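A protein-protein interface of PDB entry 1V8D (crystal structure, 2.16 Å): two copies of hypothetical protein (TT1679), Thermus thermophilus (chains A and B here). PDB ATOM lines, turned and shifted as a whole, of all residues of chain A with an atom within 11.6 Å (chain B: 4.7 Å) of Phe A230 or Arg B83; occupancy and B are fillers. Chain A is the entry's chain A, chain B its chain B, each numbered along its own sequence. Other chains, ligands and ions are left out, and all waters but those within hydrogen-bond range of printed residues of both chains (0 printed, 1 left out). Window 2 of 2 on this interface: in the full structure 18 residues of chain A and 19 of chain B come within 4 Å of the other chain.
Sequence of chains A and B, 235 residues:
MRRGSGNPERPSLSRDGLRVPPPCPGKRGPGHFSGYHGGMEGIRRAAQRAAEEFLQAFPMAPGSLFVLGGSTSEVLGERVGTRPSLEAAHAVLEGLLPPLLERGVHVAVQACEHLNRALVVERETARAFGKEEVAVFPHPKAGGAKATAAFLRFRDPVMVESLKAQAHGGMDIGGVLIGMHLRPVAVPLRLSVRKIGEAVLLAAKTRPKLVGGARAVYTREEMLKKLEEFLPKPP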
ATOM      1  N   ARG A 215      -0.197 -13.164 -20.783  1.00  0.00           N
ATOM      2  CA  ARG A 215       0.514 -14.127 -21.560  1.00  0.00           C
ATOM      3  C   ARG A 215       2.009 -13.924 -21.561  1.00  0.00           C
ATOM      4  O   ARG A 215       2.729 -14.786 -21.990  1.00  0.00           O
ATOM      5  CB  ARG A 215       0.050 -14.027 -22.997  1.00  0.00           C
ATOM      6  CG  ARG A 215      -1.267 -14.683 -23.350  1.00  0.00           C
ATOM      7  CD  ARG A 215      -1.418 -14.527 -24.861  1.00  0.00           C
ATOM      8  NE  ARG A 215      -2.421 -13.481 -24.957  1.00  0.00           N
ATOM      9  CZ  ARG A 215      -2.425 -12.427 -25.762  1.00  0.00           C
ATOM     10  NH1 ARG A 215      -1.476 -12.153 -26.670  1.00  0.00           N
ATOM     11  NH2 ARG A 215      -3.404 -11.596 -25.564  1.00  0.00           N
ATOM     12  N   GLU A 221      14.443 -18.644 -20.093  1.00  0.00           N
ATOM     13  CA  GLU A 221      14.020 -20.019 -19.917  1.00  0.00           C
ATOM     14  C   GLU A 221      12.546 -20.182 -20.301  1.00  0.00           C
ATOM     15  O   GLU A 221      12.214 -21.063 -21.116  1.00  0.00           O
ATOM     16  CB  GLU A 221      14.233 -20.464 -18.449  1.00  0.00           C
ATOM     17  CG  GLU A 221      15.611 -20.119 -17.870  1.00  0.00           C
ATOM     18  CD  GLU A 221      15.792 -18.614 -17.476  1.00  0.00           C
ATOM     19  OE1 GLU A 221      16.385 -17.845 -18.277  1.00  0.00           O
ATOM     20  OE2 GLU A 221      15.343 -18.215 -16.365  1.00  0.00           O
ATOM     21  N   GLU A 222      11.676 -19.360 -19.697  1.00  0.00           N
ATOM     22  CA  GLU A 222      10.215 -19.391 -19.991  1.00  0.00           C
ATOM     23  C   GLU A 222       9.913 -19.126 -21.452  1.00  0.00           C
ATOM     24  O   GLU A 222       8.944 -19.652 -22.007  1.00  0.00           O
ATOM     25  CB  GLU A 222       9.454 -18.356 -19.160  1.00  0.00           C
ATOM     26  CG  GLU A 222       9.071 -18.849 -17.804  1.00  0.00           C
ATOM     27  CD  GLU A 222       8.315 -20.141 -17.893  1.00  0.00           C
ATOM     28  OE1 GLU A 222       7.340 -20.227 -18.688  1.00  0.00           O
ATOM     29  OE2 GLU A 222       8.702 -21.084 -17.177  1.00  0.00           O
ATOM     30  N   MET A 223      10.739 -18.266 -22.043  1.00  0.00           N
ATOM     31  CA  MET A 223      10.647 -17.913 -23.439  1.00  0.00           C
ATOM     32  C   MET A 223      10.938 -19.134 -24.327  1.00  0.00           C
ATOM     33  O   MET A 223      10.196 -19.433 -25.255  1.00  0.00           O
ATOM     34  CB  MET A 223      11.673 -16.820 -23.786  1.00  0.00           C
ATOM     35  CG  MET A 223      11.428 -16.244 -25.179  1.00  0.00           C
ATOM     36  SD  MET A 223      12.761 -15.262 -25.786  1.00  0.00           S
ATOM     37  CE  MET A 223      14.106 -16.063 -25.156  1.00  0.00           C
ATOM     38  N   LEU A 224      12.052 -19.811 -24.072  1.00  0.00           N
ATOM     39  CA  LEU A 224      12.367 -20.966 -24.913  1.00  0.00           C
ATOM     40  C   LEU A 224      11.281 -22.041 -24.774  1.00  0.00           C
ATOM     41  O   LEU A 224      10.872 -22.585 -25.744  1.00  0.00           O
ATOM     42  CB  LEU A 224      13.773 -21.471 -24.596  1.00  0.00           C
ATOM     43  CG  LEU A 224      15.066 -20.896 -25.234  1.00  0.00           C
ATOM     44  CD1 LEU A 224      14.914 -19.532 -26.007  1.00  0.00           C
ATOM     45  CD2 LEU A 224      16.063 -20.776 -24.027  1.00  0.00           C
ATOM     46  N   LYS A 225      10.775 -22.281 -23.576  1.00  0.00           N
ATOM     47  CA  LYS A 225       9.717 -23.220 -23.382  1.00  0.00           C
ATOM     48  C   LYS A 225       8.509 -22.794 -24.206  1.00  0.00           C
ATOM     49  O   LYS A 225       7.905 -23.623 -24.920  1.00  0.00           O
ATOM     50  CB  LYS A 225       9.337 -23.280 -21.925  1.00  0.00           C
ATOM     51  CG  LYS A 225       7.979 -23.884 -21.708  1.00  0.00           C
ATOM     52  CD  LYS A 225       7.746 -24.094 -20.181  1.00  0.00           C
ATOM     53  CE  LYS A 225       6.541 -25.065 -19.866  1.00  0.00           C
ATOM     54  NZ  LYS A 225       6.891 -26.562 -20.124  1.00  0.00           N
ATOM     55  N   LYS A 226       8.107 -21.516 -24.114  1.00  0.00           N
ATOM     56  CA  LYS A 226       6.963 -21.050 -24.923  1.00  0.00           C
ATOM     57  C   LYS A 226       7.231 -21.272 -26.427  1.00  0.00           C
ATOM     58  O   LYS A 226       6.307 -21.566 -27.198  1.00  0.00           O
ATOM     59  CB  LYS A 226       6.712 -19.580 -24.621  1.00  0.00           C
ATOM     60  CG  LYS A 226       5.325 -19.292 -24.183  1.00  0.00           C
ATOM     61  CD  LYS A 226       5.104 -19.555 -22.781  1.00  0.00           C
ATOM     62  CE  LYS A 226       3.646 -19.889 -22.609  1.00  0.00           C
ATOM     63  NZ  LYS A 226       3.211 -19.774 -21.187  1.00  0.00           N
ATOM     64  N   LEU A 227       8.489 -21.164 -26.855  1.00  0.00           N
ATOM     65  CA  LEU A 227       8.828 -21.378 -28.275  1.00  0.00           C
ATOM     66  C   LEU A 227       8.747 -22.862 -28.707  1.00  0.00           C
ATOM     67  O   LEU A 227       8.507 -23.152 -29.875  1.00  0.00           O
ATOM     68  CB  LEU A 227      10.237 -20.922 -28.614  1.00  0.00           C
ATOM     69  CG  LEU A 227      10.534 -19.500 -28.986  1.00  0.00           C
ATOM     70  CD1 LEU A 227      12.019 -19.247 -28.800  1.00  0.00           C
ATOM     71  CD2 LEU A 227      10.118 -19.270 -30.395  1.00  0.00           C
ATOM     72  N   GLU A 228       9.002 -23.786 -27.783  1.00  0.00           N
ATOM     73  CA  GLU A 228       8.897 -25.216 -28.109  1.00  0.00           C
ATOM     74  C   GLU A 228       7.477 -25.417 -28.578  1.00  0.00           C
ATOM     75  O   GLU A 228       7.229 -25.759 -29.733  1.00  0.00           O
ATOM     76  CB  GLU A 228       9.138 -26.075 -26.855  1.00  0.00           C
ATOM     77  CG  GLU A 228      10.602 -26.066 -26.400  1.00  0.00           C
ATOM     78  CD  GLU A 228      10.780 -26.296 -24.888  1.00  0.00           C
ATOM     79  OE1 GLU A 228      11.948 -26.196 -24.407  1.00  0.00           O
ATOM     80  OE2 GLU A 228       9.758 -26.572 -24.181  1.00  0.00           O
ATOM     81  N   GLU A 229       6.561 -25.123 -27.648  1.00  0.00           N
ATOM     82  CA  GLU A 229       5.116 -25.234 -27.797  1.00  0.00           C
ATOM     83  C   GLU A 229       4.529 -24.581 -29.056  1.00  0.00           C
ATOM     84  O   GLU A 229       3.335 -24.699 -29.369  1.00  0.00           O
ATOM     85  CB  GLU A 229       4.444 -24.627 -26.555  1.00  0.00           C
ATOM     86  CG  GLU A 229       5.166 -24.940 -25.230  1.00  0.00           C
ATOM     87  CD  GLU A 229       4.402 -24.478 -23.968  1.00  0.00           C
ATOM     88  OE1 GLU A 229       3.561 -23.537 -24.067  1.00  0.00           O
ATOM     89  OE2 GLU A 229       4.667 -25.051 -22.870  1.00  0.00           O
ATOM     90  N   PHE A 230       5.367 -23.898 -29.793  1.00  0.00           N
ATOM     91  CA  PHE A 230       4.872 -23.212 -30.961  1.00  0.00           C
ATOM     92  C   PHE A 230       5.549 -23.882 -32.149  1.00  0.00           C
ATOM     93  O   PHE A 230       4.910 -24.276 -33.120  1.00  0.00           O
ATOM     94  CB  PHE A 230       5.285 -21.725 -30.844  1.00  0.00           C
ATOM     95  CG  PHE A 230       4.524 -20.811 -31.734  1.00  0.00           C
ATOM     96  CD1 PHE A 230       3.214 -20.482 -31.427  1.00  0.00           C
ATOM     97  CD2 PHE A 230       5.085 -20.383 -32.948  1.00  0.00           C
ATOM     98  CE1 PHE A 230       2.468 -19.758 -32.323  1.00  0.00           C
ATOM     99  CE2 PHE A 230       4.347 -19.660 -33.850  1.00  0.00           C
ATOM    100  CZ  PHE A 230       3.032 -19.344 -33.543  1.00  0.00           C
ATOM    101  N   LEU A 231       6.866 -23.984 -32.023  1.00  0.00           N
ATOM    102  CA  LEU A 231       7.739 -24.583 -33.002  1.00  0.00           C
ATOM    103  C   LEU A 231       7.371 -26.044 -33.134  1.00  0.00           C
ATOM    104  O   LEU A 231       6.621 -26.577 -32.310  1.00  0.00           O
ATOM    105  CB  LEU A 231       9.187 -24.483 -32.526  1.00  0.00           C
ATOM    106  CG  LEU A 231       9.872 -23.127 -32.520  1.00  0.00           C
ATOM    107  CD1 LEU A 231      11.290 -23.276 -32.003  1.00  0.00           C
ATOM    108  CD2 LEU A 231       9.896 -22.573 -33.920  1.00  0.00           C
ATOM    109  N   PRO A 232       7.897 -26.716 -34.171  1.00  0.00           N
ATOM    110  CA  PRO A 232       7.544 -28.133 -34.285  1.00  0.00           C
ATOM    111  C   PRO A 232       8.293 -28.813 -33.112  1.00  0.00           C
ATOM    112  O   PRO A 232       8.956 -28.058 -32.360  1.00  0.00           O
ATOM    113  CB  PRO A 232       8.101 -28.529 -35.660  1.00  0.00           C
ATOM    114  CG  PRO A 232       8.499 -27.178 -36.332  1.00  0.00           C
ATOM    115  CD  PRO A 232       8.917 -26.334 -35.169  1.00  0.00           C
ATOM    116  N   SER B  73       0.907 -13.000 -39.037  1.00  0.00           N
ATOM    117  CA  SER B  73      -0.414 -13.575 -39.251  1.00  0.00           C
ATOM    118  C   SER B  73      -1.058 -12.964 -40.498  1.00  0.00           C
ATOM    119  O   SER B  73      -1.644 -13.676 -41.381  1.00  0.00           O
ATOM    120  CB  SER B  73      -1.276 -13.293 -38.052  1.00  0.00           C
ATOM    121  OG  SER B  73      -2.512 -13.900 -38.266  1.00  0.00           O
ATOM    122  N   THR B  82      -4.967 -15.762 -37.677  1.00  0.00           N
ATOM    123  CA  THR B  82      -4.547 -15.091 -36.441  1.00  0.00           C
ATOM    124  C   THR B  82      -3.448 -15.843 -35.719  1.00  0.00           C
ATOM    125  O   THR B  82      -3.282 -15.674 -34.494  1.00  0.00           O
ATOM    126  CB  THR B  82      -5.690 -14.939 -35.403  1.00  0.00           C
ATOM    127  OG1 THR B  82      -5.824 -16.152 -34.649  1.00  0.00           O
ATOM    128  CG2 THR B  82      -7.010 -14.632 -36.106  1.00  0.00           C
ATOM    129  N   ARG B  83      -2.735 -16.696 -36.457  1.00  0.00           N
ATOM    130  CA  ARG B  83      -1.639 -17.454 -35.885  1.00  0.00           C
ATOM    131  C   ARG B  83      -0.311 -16.927 -36.420  1.00  0.00           C
ATOM    132  O   ARG B  83      -0.105 -16.868 -37.615  1.00  0.00           O
ATOM    133  CB  ARG B  83      -1.745 -18.920 -36.216  1.00  0.00           C
ATOM    134  CG  ARG B  83      -0.726 -19.696 -35.472  1.00  0.00           C
ATOM    135  CD  ARG B  83      -0.801 -21.185 -35.805  1.00  0.00           C
ATOM    136  NE  ARG B  83       0.082 -21.971 -34.925  1.00  0.00           N
ATOM    137  CZ  ARG B  83       1.402 -22.137 -35.073  1.00  0.00           C
ATOM    138  NH1 ARG B  83       2.082 -21.575 -36.090  1.00  0.00           N
ATOM    139  NH2 ARG B  83       2.042 -22.904 -34.184  1.00  0.00           N
ATOM    140  N   PRO B  84       0.610 -16.520 -35.514  1.00  0.00           N
ATOM    141  CA  PRO B  84       1.929 -15.993 -35.924  1.00  0.00           C
ATOM    142  C   PRO B  84       2.746 -17.094 -36.647  1.00  0.00           C
ATOM    143  O   PRO B  84       2.460 -18.255 -36.479  1.00  0.00           O
ATOM    144  CB  PRO B  84       2.567 -15.600 -34.580  1.00  0.00           C
ATOM    145  CG  PRO B  84       1.402 -15.454 -33.616  1.00  0.00           C
ATOM    146  CD  PRO B  84       0.456 -16.508 -34.036  1.00  0.00           C
ATOM    147  N   SER B  85       3.743 -16.722 -37.443  1.00  0.00           N
ATOM    148  CA  SER B  85       4.631 -17.671 -38.127  1.00  0.00           C
ATOM    149  C   SER B  85       6.146 -17.224 -38.056  1.00  0.00           C
ATOM    150  O   SER B  85       6.550 -16.228 -38.691  1.00  0.00           O
ATOM    151  CB  SER B  85       4.186 -17.819 -39.608  1.00  0.00           C
ATOM    152  OG  SER B  85       5.251 -18.240 -40.474  1.00  0.00           O
ATOM    153  N   LEU B  86       6.970 -17.980 -37.312  1.00  0.00           N
ATOM    154  CA  LEU B  86       8.380 -17.700 -37.229  1.00  0.00           C
ATOM    155  C   LEU B  86       9.026 -17.794 -38.595  1.00  0.00           C
ATOM    156  O   LEU B  86       9.979 -17.051 -38.890  1.00  0.00           O
ATOM    157  CB  LEU B  86       9.056 -18.651 -36.276  1.00  0.00           C
ATOM    158  CG  LEU B  86       8.765 -18.291 -34.853  1.00  0.00           C
ATOM    159  CD1 LEU B  86       9.384 -19.319 -33.940  1.00  0.00           C
ATOM    160  CD2 LEU B  86       9.431 -16.940 -34.553  1.00  0.00           C
ATOM    161  N   PRO B 140       6.086 -15.756 -29.668  1.00  0.00           N
ATOM    162  CA  PRO B 140       4.993 -15.515 -30.626  1.00  0.00           C
ATOM    163  C   PRO B 140       3.620 -15.205 -30.122  1.00  0.00           C
ATOM    164  O   PRO B 140       2.982 -14.352 -30.679  1.00  0.00           O
ATOM    165  CB  PRO B 140       5.001 -16.753 -31.535  1.00  0.00           C
ATOM    166  CG  PRO B 140       6.484 -17.172 -31.488  1.00  0.00           C
ATOM    167  CD  PRO B 140       6.839 -16.982 -30.004  1.00  0.00           C
ATOM    168  N   LYS B 141       3.130 -15.874 -29.094  1.00  0.00           N
ATOM    169  CA  LYS B 141       1.763 -15.599 -28.589  1.00  0.00           C
ATOM    170  C   LYS B 141       1.656 -14.390 -27.646  1.00  0.00           C
ATOM    171  O   LYS B 141       0.564 -14.113 -27.150  1.00  0.00           O
ATOM    172  CB  LYS B 141       1.175 -16.817 -27.858  1.00  0.00           C
ATOM    173  CG  LYS B 141       0.474 -17.835 -28.761  1.00  0.00           C
ATOM    174  CD  LYS B 141       0.401 -19.239 -28.127  1.00  0.00           C
ATOM    175  CE  LYS B 141       0.415 -20.368 -29.227  1.00  0.00           C
ATOM    176  NZ  LYS B 141       0.147 -21.731 -28.607  1.00  0.00           N
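NH1 of Arg A215 is in hydrogen-bond range of O of Lys B141, at 2.9 Å. The backbone carbonyl oxygen of Phe A230 is in hydrogen-bond range of the guanidinium group of Arg B83 (3.4 Å).
The side-chain hydroxyl of Ser B73 lies within hydrogen-bond range of the backbone NH of Arg B83 (3.3 Å).
Among the printed residues, merely in contact across the chains: Leu A227 with Leu B86, Phe A230 with Pro B84, Phe A230 with Pro B140, Phe A230 with Lys B141 and Leu A231 with Leu B86.
Phe A230 touches just these residues of chain B: Arg B83, Pro B84, Pro B140 and Lys B141. Arg B83 touches one residue of chain A. No residue of chain A comes within 4 Å of Ser B73. No residue of chain A comes within 4 Å of Thr B82. Printed residues of chain A within 4 Å of Pro B84: Phe A230 (3.2 Å). No residue of chain A comes within 4 Å of Ser B85. Of the printed residues of chain B, Leu A227 touches Leu B86 (3.6 Å). Of the printed residues of chain B, Leu A231 touches Leu B86 (3.3 Å). Of the printed residues of chain B, Arg A215 touches Lys B141. Glu A222 touches none of the printed residues of chain B. The nearest residue of chain A that does not touch Arg B83 is Glu A229 (5.3 Å).
Of the 13 printed residues of chain A, 4 touch a printed residue of chain B. Printed residues of chain A that touch a printed residue of chain B: Arg A215, Leu A227, Phe A230 and Leu A231. Hydrophobic or aromatic side chains of chain A that line the printed part of chain B: Leu A227, Phe A230 and Leu A231. Among the printed residues, 7 pairs touch across the chains. Among the printed residues, no Asp or Glu carboxylate lies within 4 Å of a Lys or Arg side-chain nitrogen of the other chain.
No position is printed for both chains.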
